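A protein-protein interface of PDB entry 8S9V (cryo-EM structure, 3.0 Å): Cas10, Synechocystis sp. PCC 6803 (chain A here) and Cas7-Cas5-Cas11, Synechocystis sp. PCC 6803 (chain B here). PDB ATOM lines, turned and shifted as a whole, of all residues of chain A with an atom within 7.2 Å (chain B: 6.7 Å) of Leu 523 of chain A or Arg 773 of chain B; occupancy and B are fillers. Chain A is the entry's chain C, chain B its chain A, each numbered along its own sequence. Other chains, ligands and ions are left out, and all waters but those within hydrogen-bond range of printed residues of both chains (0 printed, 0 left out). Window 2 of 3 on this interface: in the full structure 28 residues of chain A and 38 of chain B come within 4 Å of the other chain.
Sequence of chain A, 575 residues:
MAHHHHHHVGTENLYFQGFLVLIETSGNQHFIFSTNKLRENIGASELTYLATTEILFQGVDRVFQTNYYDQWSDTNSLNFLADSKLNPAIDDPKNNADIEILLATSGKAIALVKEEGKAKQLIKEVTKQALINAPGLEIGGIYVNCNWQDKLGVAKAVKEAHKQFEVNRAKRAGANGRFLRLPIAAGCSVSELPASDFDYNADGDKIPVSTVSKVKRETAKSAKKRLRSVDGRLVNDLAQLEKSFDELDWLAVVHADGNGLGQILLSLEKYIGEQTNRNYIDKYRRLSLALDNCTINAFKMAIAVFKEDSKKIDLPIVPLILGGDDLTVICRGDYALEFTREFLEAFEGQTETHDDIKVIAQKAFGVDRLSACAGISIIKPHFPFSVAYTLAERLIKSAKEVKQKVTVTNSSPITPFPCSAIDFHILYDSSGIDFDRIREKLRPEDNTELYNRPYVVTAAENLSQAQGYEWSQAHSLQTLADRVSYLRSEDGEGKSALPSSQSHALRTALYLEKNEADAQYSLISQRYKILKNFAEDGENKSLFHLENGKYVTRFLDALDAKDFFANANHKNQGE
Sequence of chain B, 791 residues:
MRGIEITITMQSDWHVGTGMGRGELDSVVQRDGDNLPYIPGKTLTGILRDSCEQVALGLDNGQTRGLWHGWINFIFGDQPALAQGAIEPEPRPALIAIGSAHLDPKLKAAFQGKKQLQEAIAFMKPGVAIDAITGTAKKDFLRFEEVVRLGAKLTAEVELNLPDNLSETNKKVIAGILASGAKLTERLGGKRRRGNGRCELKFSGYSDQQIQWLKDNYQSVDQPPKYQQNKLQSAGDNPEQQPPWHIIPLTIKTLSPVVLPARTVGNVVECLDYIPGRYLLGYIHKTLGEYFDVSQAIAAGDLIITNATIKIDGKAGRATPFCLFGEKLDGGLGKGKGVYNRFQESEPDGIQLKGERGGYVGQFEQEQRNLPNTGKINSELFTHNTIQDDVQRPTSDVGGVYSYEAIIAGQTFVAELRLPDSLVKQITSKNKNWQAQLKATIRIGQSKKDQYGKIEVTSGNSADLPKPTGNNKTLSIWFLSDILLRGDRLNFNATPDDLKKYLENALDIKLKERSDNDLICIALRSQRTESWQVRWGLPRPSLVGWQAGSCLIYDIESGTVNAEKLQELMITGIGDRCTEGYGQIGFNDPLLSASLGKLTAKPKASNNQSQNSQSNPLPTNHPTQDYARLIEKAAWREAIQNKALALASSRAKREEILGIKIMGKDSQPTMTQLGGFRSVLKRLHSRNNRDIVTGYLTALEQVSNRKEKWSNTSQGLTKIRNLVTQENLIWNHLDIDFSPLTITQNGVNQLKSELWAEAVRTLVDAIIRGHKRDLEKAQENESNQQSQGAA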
ATOM      1  N   GLN A 502     -20.223 -20.703 -10.939  1.00  0.00           N
ATOM      2  CA  GLN A 502     -19.245 -20.074 -10.058  1.00  0.00           C
ATOM      3  C   GLN A 502     -19.175 -20.701  -8.676  1.00  0.00           C
ATOM      4  O   GLN A 502     -18.101 -20.737  -8.083  1.00  0.00           O
ATOM      5  CB  GLN A 502     -19.528 -18.584  -9.914  1.00  0.00           C
ATOM      6  CG  GLN A 502     -19.485 -17.836 -11.197  1.00  0.00           C
ATOM      7  CD  GLN A 502     -18.123 -17.871 -11.807  1.00  0.00           C
ATOM      8  OE1 GLN A 502     -17.137 -17.991 -11.110  1.00  0.00           O
ATOM      9  NE2 GLN A 502     -18.056 -17.779 -13.109  1.00  0.00           N
ATOM     10  N   ALA A 517      -7.374 -21.005  -1.803  1.00  0.00           N
ATOM     11  CA  ALA A 517      -8.816 -20.834  -1.700  1.00  0.00           C
ATOM     12  C   ALA A 517      -9.204 -19.362  -1.678  1.00  0.00           C
ATOM     13  O   ALA A 517     -10.144 -18.951  -2.359  1.00  0.00           O
ATOM     14  CB  ALA A 517      -9.327 -21.549  -0.459  1.00  0.00           C
ATOM     15  N   ASP A 518      -8.513 -18.558  -0.875  1.00  0.00           N
ATOM     16  CA  ASP A 518      -8.731 -17.116  -0.858  1.00  0.00           C
ATOM     17  C   ASP A 518      -8.347 -16.447  -2.167  1.00  0.00           C
ATOM     18  O   ASP A 518      -8.941 -15.436  -2.541  1.00  0.00           O
ATOM     19  CB  ASP A 518      -7.939 -16.485   0.268  1.00  0.00           C
ATOM     20  CG  ASP A 518      -8.427 -16.904   1.608  1.00  0.00           C
ATOM     21  OD1 ASP A 518      -9.489 -17.544   1.667  1.00  0.00           O
ATOM     22  OD2 ASP A 518      -7.763 -16.583   2.610  1.00  0.00           O
ATOM     23  N   ALA A 519      -7.329 -16.959  -2.844  1.00  0.00           N
ATOM     24  CA  ALA A 519      -6.973 -16.458  -4.162  1.00  0.00           C
ATOM     25  C   ALA A 519      -8.121 -16.591  -5.148  1.00  0.00           C
ATOM     26  O   ALA A 519      -8.393 -15.670  -5.920  1.00  0.00           O
ATOM     27  CB  ALA A 519      -5.737 -17.186  -4.664  1.00  0.00           C
ATOM     28  N   GLN A 520      -8.750 -17.759  -5.208  1.00  0.00           N
ATOM     29  CA  GLN A 520      -9.878 -17.946  -6.115  1.00  0.00           C
ATOM     30  C   GLN A 520     -11.080 -17.082  -5.771  1.00  0.00           C
ATOM     31  O   GLN A 520     -11.762 -16.585  -6.667  1.00  0.00           O
ATOM     32  CB  GLN A 520     -10.309 -19.405  -6.122  1.00  0.00           C
ATOM     33  CG  GLN A 520      -9.936 -20.127  -7.362  1.00  0.00           C
ATOM     34  CD  GLN A 520     -10.887 -19.790  -8.459  1.00  0.00           C
ATOM     35  OE1 GLN A 520     -11.890 -19.122  -8.233  1.00  0.00           O
ATOM     36  NE2 GLN A 520     -10.585 -20.240  -9.659  1.00  0.00           N
ATOM     37  N   TYR A 521     -11.370 -16.899  -4.492  1.00  0.00           N
ATOM     38  CA  TYR A 521     -12.455 -16.012  -4.107  1.00  0.00           C
ATOM     39  C   TYR A 521     -12.182 -14.577  -4.515  1.00  0.00           C
ATOM     40  O   TYR A 521     -13.075 -13.876  -4.991  1.00  0.00           O
ATOM     41  CB  TYR A 521     -12.665 -16.112  -2.608  1.00  0.00           C
ATOM     42  CG  TYR A 521     -13.737 -15.238  -2.035  1.00  0.00           C
ATOM     43  CD1 TYR A 521     -15.037 -15.669  -1.985  1.00  0.00           C
ATOM     44  CD2 TYR A 521     -13.450 -14.007  -1.520  1.00  0.00           C
ATOM     45  CE1 TYR A 521     -16.012 -14.902  -1.443  1.00  0.00           C
ATOM     46  CE2 TYR A 521     -14.428 -13.228  -0.986  1.00  0.00           C
ATOM     47  CZ  TYR A 521     -15.705 -13.680  -0.949  1.00  0.00           C
ATOM     48  OH  TYR A 521     -16.684 -12.903  -0.406  1.00  0.00           O
ATOM     49  N   SER A 522     -10.948 -14.127  -4.359  1.00  0.00           N
ATOM     50  CA  SER A 522     -10.589 -12.772  -4.734  1.00  0.00           C
ATOM     51  C   SER A 522     -10.676 -12.538  -6.228  1.00  0.00           C
ATOM     52  O   SER A 522     -10.714 -11.387  -6.658  1.00  0.00           O
ATOM     53  CB  SER A 522      -9.192 -12.476  -4.234  1.00  0.00           C
ATOM     54  OG  SER A 522      -9.130 -12.670  -2.837  1.00  0.00           O
ATOM     55  N   LEU A 523     -10.661 -13.594  -7.029  1.00  0.00           N
ATOM     56  CA  LEU A 523     -10.944 -13.461  -8.446  1.00  0.00           C
ATOM     57  C   LEU A 523     -12.414 -13.212  -8.726  1.00  0.00           C
ATOM     58  O   LEU A 523     -12.748 -12.759  -9.821  1.00  0.00           O
ATOM     59  CB  LEU A 523     -10.497 -14.724  -9.175  1.00  0.00           C
ATOM     60  CG  LEU A 523      -9.132 -14.737  -9.844  1.00  0.00           C
ATOM     61  CD1 LEU A 523      -8.075 -14.650  -8.801  1.00  0.00           C
ATOM     62  CD2 LEU A 523      -8.968 -16.000 -10.602  1.00  0.00           C
ATOM     63  N   ILE A 524     -13.291 -13.468  -7.760  1.00  0.00           N
ATOM     64  CA  ILE A 524     -14.733 -13.523  -7.977  1.00  0.00           C
ATOM     65  C   ILE A 524     -15.436 -12.469  -7.148  1.00  0.00           C
ATOM     66  O   ILE A 524     -16.458 -11.921  -7.558  1.00  0.00           O
ATOM     67  CB  ILE A 524     -15.302 -14.905  -7.625  1.00  0.00           C
ATOM     68  CG1 ILE A 524     -14.668 -15.991  -8.461  1.00  0.00           C
ATOM     69  CG2 ILE A 524     -16.759 -14.947  -7.859  1.00  0.00           C
ATOM     70  CD1 ILE A 524     -15.151 -17.334  -8.084  1.00  0.00           C
ATOM     71  N   SER A 525     -14.862 -12.142  -6.002  1.00  0.00           N
ATOM     72  CA  SER A 525     -15.598 -11.483  -4.939  1.00  0.00           C
ATOM     73  C   SER A 525     -16.239 -10.176  -5.362  1.00  0.00           C
ATOM     74  O   SER A 525     -17.212  -9.758  -4.734  1.00  0.00           O
ATOM     75  CB  SER A 525     -14.671 -11.238  -3.759  1.00  0.00           C
ATOM     76  OG  SER A 525     -13.667 -10.311  -4.103  1.00  0.00           O
ATOM     77  N   GLN A 526     -15.729  -9.507  -6.391  1.00  0.00           N
ATOM     78  CA  GLN A 526     -16.373  -8.286  -6.853  1.00  0.00           C
ATOM     79  C   GLN A 526     -17.274  -8.470  -8.053  1.00  0.00           C
ATOM     80  O   GLN A 526     -18.090  -7.590  -8.330  1.00  0.00           O
ATOM     81  CB  GLN A 526     -15.319  -7.249  -7.240  1.00  0.00           C
ATOM     82  CG  GLN A 526     -14.602  -6.616  -6.063  1.00  0.00           C
ATOM     83  CD  GLN A 526     -15.457  -5.654  -5.286  1.00  0.00           C
ATOM     84  OE1 GLN A 526     -15.747  -5.882  -4.115  1.00  0.00           O
ATOM     85  NE2 GLN A 526     -15.862  -4.564  -5.927  1.00  0.00           N
ATOM     86  N   ARG A 527     -17.158  -9.578  -8.762  1.00  0.00           N
ATOM     87  CA  ARG A 527     -18.065  -9.864  -9.862  1.00  0.00           C
ATOM     88  C   ARG A 527     -19.459 -10.246  -9.403  1.00  0.00           C
ATOM     89  O   ARG A 527     -20.424 -10.027 -10.137  1.00  0.00           O
ATOM     90  CB  ARG A 527     -17.467 -10.967 -10.705  1.00  0.00           C
ATOM     91  CG  ARG A 527     -16.325 -10.517 -11.534  1.00  0.00           C
ATOM     92  CD  ARG A 527     -15.949 -11.620 -12.425  1.00  0.00           C
ATOM     93  NE  ARG A 527     -15.049 -11.232 -13.481  1.00  0.00           N
ATOM     94  CZ  ARG A 527     -15.025 -11.847 -14.644  1.00  0.00           C
ATOM     95  NH1 ARG A 527     -14.273 -11.400 -15.632  1.00  0.00           N
ATOM     96  NH2 ARG A 527     -15.833 -12.874 -14.832  1.00  0.00           N
ATOM     97  N   TYR A 528     -19.599 -10.798  -8.203  1.00  0.00           N
ATOM     98  CA  TYR A 528     -20.888 -11.271  -7.714  1.00  0.00           C
ATOM     99  C   TYR A 528     -21.173 -10.658  -6.356  1.00  0.00           C
ATOM    100  O   TYR A 528     -20.732 -11.161  -5.325  1.00  0.00           O
ATOM    101  CB  TYR A 528     -20.905 -12.796  -7.676  1.00  0.00           C
ATOM    102  CG  TYR A 528     -20.631 -13.365  -9.045  1.00  0.00           C
ATOM    103  CD1 TYR A 528     -19.346 -13.602  -9.467  1.00  0.00           C
ATOM    104  CD2 TYR A 528     -21.648 -13.548  -9.952  1.00  0.00           C
ATOM    105  CE1 TYR A 528     -19.096 -14.069 -10.709  1.00  0.00           C
ATOM    106  CE2 TYR A 528     -21.397 -14.004 -11.192  1.00  0.00           C
ATOM    107  CZ  TYR A 528     -20.122 -14.261 -11.566  1.00  0.00           C
ATOM    108  OH  TYR A 528     -19.868 -14.718 -12.823  1.00  0.00           O
ATOM    109  N   LEU A 531     -21.712 -12.246  -3.002  1.00  0.00           N
ATOM    110  CA  LEU A 531     -20.643 -12.907  -2.265  1.00  0.00           C
ATOM    111  C   LEU A 531     -20.227 -12.184  -1.000  1.00  0.00           C
ATOM    112  O   LEU A 531     -19.581 -12.790  -0.146  1.00  0.00           O
ATOM    113  CB  LEU A 531     -19.421 -13.065  -3.157  1.00  0.00           C
ATOM    114  CG  LEU A 531     -19.462 -14.108  -4.252  1.00  0.00           C
ATOM    115  CD1 LEU A 531     -18.215 -14.001  -5.037  1.00  0.00           C
ATOM    116  CD2 LEU A 531     -19.545 -15.445  -3.605  1.00  0.00           C
ATOM    117  N   LEU B 645      -1.393 -19.693  -8.525  1.00  0.00           N
ATOM    118  CA  LEU B 645      -2.622 -19.041  -8.072  1.00  0.00           C
ATOM    119  C   LEU B 645      -2.408 -18.202  -6.826  1.00  0.00           C
ATOM    120  O   LEU B 645      -2.947 -17.099  -6.717  1.00  0.00           O
ATOM    121  CB  LEU B 645      -3.697 -20.076  -7.774  1.00  0.00           C
ATOM    122  CG  LEU B 645      -5.070 -19.993  -8.421  1.00  0.00           C
ATOM    123  CD1 LEU B 645      -5.869 -21.151  -7.917  1.00  0.00           C
ATOM    124  CD2 LEU B 645      -5.768 -18.712  -8.127  1.00  0.00           C
ATOM    125  N   ALA B 648      -0.255 -14.905  -7.571  1.00  0.00           N
ATOM    126  CA  ALA B 648      -1.017 -13.867  -8.245  1.00  0.00           C
ATOM    127  C   ALA B 648      -1.976 -13.136  -7.330  1.00  0.00           C
ATOM    128  O   ALA B 648      -2.435 -12.054  -7.682  1.00  0.00           O
ATOM    129  CB  ALA B 648      -1.780 -14.462  -9.411  1.00  0.00           C
ATOM    130  N   SER B 649      -2.309 -13.703  -6.181  1.00  0.00           N
ATOM    131  CA  SER B 649      -3.372 -13.141  -5.364  1.00  0.00           C
ATOM    132  C   SER B 649      -2.960 -11.856  -4.685  1.00  0.00           C
ATOM    133  O   SER B 649      -3.829 -11.138  -4.188  1.00  0.00           O
ATOM    134  CB  SER B 649      -3.836 -14.131  -4.313  1.00  0.00           C
ATOM    135  OG  SER B 649      -2.883 -14.246  -3.279  1.00  0.00           O
ATOM    136  N   MET B 671      -3.753  -3.025 -19.826  1.00  0.00           N
ATOM    137  CA  MET B 671      -4.034  -4.440 -19.988  1.00  0.00           C
ATOM    138  C   MET B 671      -3.762  -4.896 -21.407  1.00  0.00           C
ATOM    139  O   MET B 671      -3.418  -6.055 -21.626  1.00  0.00           O
ATOM    140  CB  MET B 671      -5.480  -4.740 -19.626  1.00  0.00           C
ATOM    141  CG  MET B 671      -5.792  -4.708 -18.169  1.00  0.00           C
ATOM    142  SD  MET B 671      -4.840  -5.820 -17.147  1.00  0.00           S
ATOM    143  CE  MET B 671      -4.915  -7.323 -18.086  1.00  0.00           C
ATOM    144  N   ALA B 766      -1.202 -16.708 -14.643  1.00  0.00           N
ATOM    145  CA  ALA B 766      -1.832 -16.453 -13.353  1.00  0.00           C
ATOM    146  C   ALA B 766      -1.706 -15.006 -12.914  1.00  0.00           C
ATOM    147  O   ALA B 766      -2.649 -14.429 -12.375  1.00  0.00           O
ATOM    148  CB  ALA B 766      -1.240 -17.372 -12.299  1.00  0.00           C
ATOM    149  N   ILE B 768      -1.239 -12.231 -14.702  1.00  0.00           N
ATOM    150  CA  ILE B 768      -2.044 -11.295 -15.477  1.00  0.00           C
ATOM    151  C   ILE B 768      -3.525 -11.446 -15.170  1.00  0.00           C
ATOM    152  O   ILE B 768      -4.264 -10.466 -15.180  1.00  0.00           O
ATOM    153  CB  ILE B 768      -1.770 -11.437 -16.974  1.00  0.00           C
ATOM    154  CG1 ILE B 768      -0.352 -11.018 -17.288  1.00  0.00           C
ATOM    155  CG2 ILE B 768      -2.695 -10.573 -17.729  1.00  0.00           C
ATOM    156  CD1 ILE B 768       0.043 -11.322 -18.683  1.00  0.00           C
ATOM    157  N   ARG B 769      -4.000 -12.664 -14.948  1.00  0.00           N
ATOM    158  CA  ARG B 769      -5.385 -12.831 -14.526  1.00  0.00           C
ATOM    159  C   ARG B 769      -5.639 -12.171 -13.189  1.00  0.00           C
ATOM    160  O   ARG B 769      -6.610 -11.435 -13.028  1.00  0.00           O
ATOM    161  CB  ARG B 769      -5.747 -14.305 -14.427  1.00  0.00           C
ATOM    162  CG  ARG B 769      -7.202 -14.513 -14.127  1.00  0.00           C
ATOM    163  CD  ARG B 769      -7.596 -15.960 -14.089  1.00  0.00           C
ATOM    164  NE  ARG B 769      -7.400 -16.609 -15.367  1.00  0.00           N
ATOM    165  CZ  ARG B 769      -6.403 -17.435 -15.641  1.00  0.00           C
ATOM    166  NH1 ARG B 769      -6.156 -17.802 -16.882  1.00  0.00           N
ATOM    167  NH2 ARG B 769      -5.594 -17.818 -14.670  1.00  0.00           N
ATOM    168  N   GLY B 770      -4.789 -12.443 -12.206  1.00  0.00           N
ATOM    169  CA  GLY B 770      -4.960 -11.838 -10.899  1.00  0.00           C
ATOM    170  C   GLY B 770      -4.860 -10.335 -10.921  1.00  0.00           C
ATOM    171  O   GLY B 770      -5.564  -9.649 -10.191  1.00  0.00           O
ATOM    172  N   HIS B 771      -3.981  -9.805 -11.756  1.00  0.00           N
ATOM    173  CA  HIS B 771      -3.896  -8.365 -11.963  1.00  0.00           C
ATOM    174  C   HIS B 771      -5.202  -7.801 -12.479  1.00  0.00           C
ATOM    175  O   HIS B 771      -5.746  -6.856 -11.912  1.00  0.00           O
ATOM    176  CB  HIS B 771      -2.769  -8.074 -12.943  1.00  0.00           C
ATOM    177  CG  HIS B 771      -2.663  -6.645 -13.366  1.00  0.00           C
ATOM    178  ND1 HIS B 771      -2.481  -5.615 -12.478  1.00  0.00           N
ATOM    179  CD2 HIS B 771      -2.638  -6.086 -14.594  1.00  0.00           C
ATOM    180  CE1 HIS B 771      -2.379  -4.480 -13.139  1.00  0.00           C
ATOM    181  NE2 HIS B 771      -2.477  -4.737 -14.424  1.00  0.00           N
ATOM    182  N   LYS B 772      -5.732  -8.379 -13.547  1.00  0.00           N
ATOM    183  CA  LYS B 772      -6.932  -7.833 -14.158  1.00  0.00           C
ATOM    184  C   LYS B 772      -8.117  -7.847 -13.214  1.00  0.00           C
ATOM    185  O   LYS B 772      -8.907  -6.906 -13.198  1.00  0.00           O
ATOM    186  CB  LYS B 772      -7.269  -8.604 -15.420  1.00  0.00           C
ATOM    187  CG  LYS B 772      -7.992  -7.767 -16.429  1.00  0.00           C
ATOM    188  CD  LYS B 772      -9.446  -7.739 -16.176  1.00  0.00           C
ATOM    189  CE  LYS B 772     -10.093  -6.680 -16.986  1.00  0.00           C
ATOM    190  NZ  LYS B 772     -11.541  -6.920 -17.017  1.00  0.00           N
ATOM    191  N   ARG B 773      -8.300  -8.914 -12.465  1.00  0.00           N
ATOM    192  CA  ARG B 773      -9.416  -8.970 -11.533  1.00  0.00           C
ATOM    193  C   ARG B 773      -9.214  -8.190 -10.246  1.00  0.00           C
ATOM    194  O   ARG B 773     -10.157  -8.078  -9.470  1.00  0.00           O
ATOM    195  CB  ARG B 773      -9.747 -10.416 -11.237  1.00  0.00           C
ATOM    196  CG  ARG B 773     -10.057 -11.115 -12.516  1.00  0.00           C
ATOM    197  CD  ARG B 773     -10.953 -12.261 -12.317  1.00  0.00           C
ATOM    198  NE  ARG B 773     -11.075 -13.010 -13.546  1.00  0.00           N
ATOM    199  CZ  ARG B 773     -11.960 -13.971 -13.732  1.00  0.00           C
ATOM    200  NH1 ARG B 773     -11.999 -14.609 -14.883  1.00  0.00           N
ATOM    201  NH2 ARG B 773     -12.789 -14.309 -12.764  1.00  0.00           N
ATOM    202  N   ASP B 774      -8.038  -7.637 -10.002  1.00  0.00           N
ATOM    203  CA  ASP B 774      -7.895  -6.592  -9.005  1.00  0.00           C
ATOM    204  C   ASP B 774      -8.037  -5.217  -9.619  1.00  0.00           C
ATOM    205  O   ASP B 774      -8.512  -4.292  -8.961  1.00  0.00           O
ATOM    206  CB  ASP B 774      -6.544  -6.689  -8.307  1.00  0.00           C
ATOM    207  CG  ASP B 774      -6.485  -7.825  -7.315  1.00  0.00           C
ATOM    208  OD1 ASP B 774      -7.529  -8.453  -7.075  1.00  0.00           O
ATOM    209  OD2 ASP B 774      -5.399  -8.087  -6.755  1.00  0.00           O
ATOM    210  N   LEU B 775      -7.588  -5.062 -10.851  1.00  0.00           N
ATOM    211  CA  LEU B 775      -7.853  -3.843 -11.595  1.00  0.00           C
ATOM    212  C   LEU B 775      -9.339  -3.551 -11.697  1.00  0.00           C
ATOM    213  O   LEU B 775      -9.750  -2.392 -11.630  1.00  0.00           O
ATOM    214  CB  LEU B 775      -7.247  -3.970 -12.978  1.00  0.00           C
ATOM    215  CG  LEU B 775      -7.474  -2.815 -13.898  1.00  0.00           C
ATOM    216  CD1 LEU B 775      -6.875  -1.636 -13.255  1.00  0.00           C
ATOM    217  CD2 LEU B 775      -6.755  -3.130 -15.138  1.00  0.00           C
ATOM    218  N   GLU B 776     -10.155  -4.575 -11.903  1.00  0.00           N
ATOM    219  CA  GLU B 776     -11.600  -4.395 -11.902  1.00  0.00           C
ATOM    220  C   GLU B 776     -12.122  -3.837 -10.589  1.00  0.00           C
ATOM    221  O   GLU B 776     -13.113  -3.108 -10.585  1.00  0.00           O
ATOM    222  CB  GLU B 776     -12.280  -5.725 -12.170  1.00  0.00           C
ATOM    223  CG  GLU B 776     -12.199  -6.235 -13.572  1.00  0.00           C
ATOM    224  CD  GLU B 776     -12.823  -7.605 -13.685  1.00  0.00           C
ATOM    225  OE1 GLU B 776     -13.359  -8.084 -12.671  1.00  0.00           O
ATOM    226  OE2 GLU B 776     -12.766  -8.215 -14.769  1.00  0.00           O
ATOM    227  N   LYS B 777     -11.499  -4.184  -9.468  1.00  0.00           N
ATOM    228  CA  LYS B 777     -11.933  -3.641  -8.187  1.00  0.00           C
ATOM    229  C   LYS B 777     -11.586  -2.169  -8.042  1.00  0.00           C
ATOM    230  O   LYS B 777     -12.412  -1.376  -7.590  1.00  0.00           O
ATOM    231  CB  LYS B 777     -11.330  -4.439  -7.037  1.00  0.00           C
ATOM    232  CG  LYS B 777     -11.540  -5.924  -7.095  1.00  0.00           C
ATOM    233  CD  LYS B 777     -11.106  -6.530  -5.788  1.00  0.00           C
ATOM    234  CE  LYS B 777     -11.368  -8.009  -5.707  1.00  0.00           C
ATOM    235  NZ  LYS B 777     -10.569  -8.798  -6.634  1.00  0.00           N
ATOM    236  N   ALA B 778     -10.366  -1.782  -8.402  1.00  0.00           N
ATOM    237  CA  ALA B 778      -9.993  -0.376  -8.317  1.00  0.00           C
ATOM    238  C   ALA B 778     -10.783   0.452  -9.309  1.00  0.00           C
ATOM    239  O   ALA B 778     -11.196   1.573  -9.006  1.00  0.00           O
ATOM    240  CB  ALA B 778      -8.502  -0.217  -8.574  1.00  0.00           C
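The side-chain amino group (NZ) of Lys 777 of chain B is in hydrogen-bond range of the backbone carbonyl oxygen (O) of Ser 522 of chain A, at 2.6 Å.
The guanidinium group (NH1) of Arg 527 of chain A is in salt-bridge range of the side-chain carboxylate (OE2) of Glu 776 of chain B, at 3.6 Å.
O of Leu 523 of chain A sits close to NH2 of Arg 773 of chain B (3.3 Å).
The side-chain amino group (NZ) of Lys 772 of chain B is in salt-bridge range of the side-chain carboxylate (OE2) of Glu 776 of chain B.
O of Arg 773 of chain B lies within hydrogen-bond range of NZ of Lys 777 of chain B (3.0 Å).
The side-chain carboxylate (OD1) of Asp 774 of chain B is in salt-bridge range of the side-chain amino group (NZ) of Lys 777 of chain B (3.1 Å).
O of Asp 518 of chain A sits at hydrogen-bond distance from OG of Ser 522 of chain A, at 2.8 Å.
CB of Ala 519 of chain A touches O of Leu 645 of chain B (3.5 Å).
Ser 649 of chain B touches Ala 519 of chain A (CB to CB, 3.6 Å).
CD2 of Leu 523 of chain A touches CD of Arg 769 of chain B, 3.7 Å away.
Ser 525 of chain A touches Lys 777 of chain B.
Lys 777 of chain B touches Gln 526 of chain A.
Arg 527 of chain A touches Arg 773 of chain B.
Of the printed residues of chain B, Ser 522 of chain A touches Lys 777.
Leu 523 of chain A touches just these residues of chain B: Arg 769 (3.7 Å) and Arg 773 (3.1 Å).
Printed residues of chain B within 4 Å of Gln 526 of chain A: Lys 777 (3.3 Å).
Printed residues of chain B within 4 Å of Arg 527 of chain A: Arg 773 and Glu 776.
Of chain A, only Leu 523 (3.1 Å) and Arg 527 (3.8 Å) come within 4 Å of Arg 773 of chain B.
Of the 16 printed residues of chain B, 6 touch a printed residue of chain A.
Of the 14 printed residues of chain A, 6 touch a printed residue of chain B.
Along chain A the printed residues that touch a printed residue of chain B span positions 519 to 527.
Among the printed residues, 9 pairs touch across the chains.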
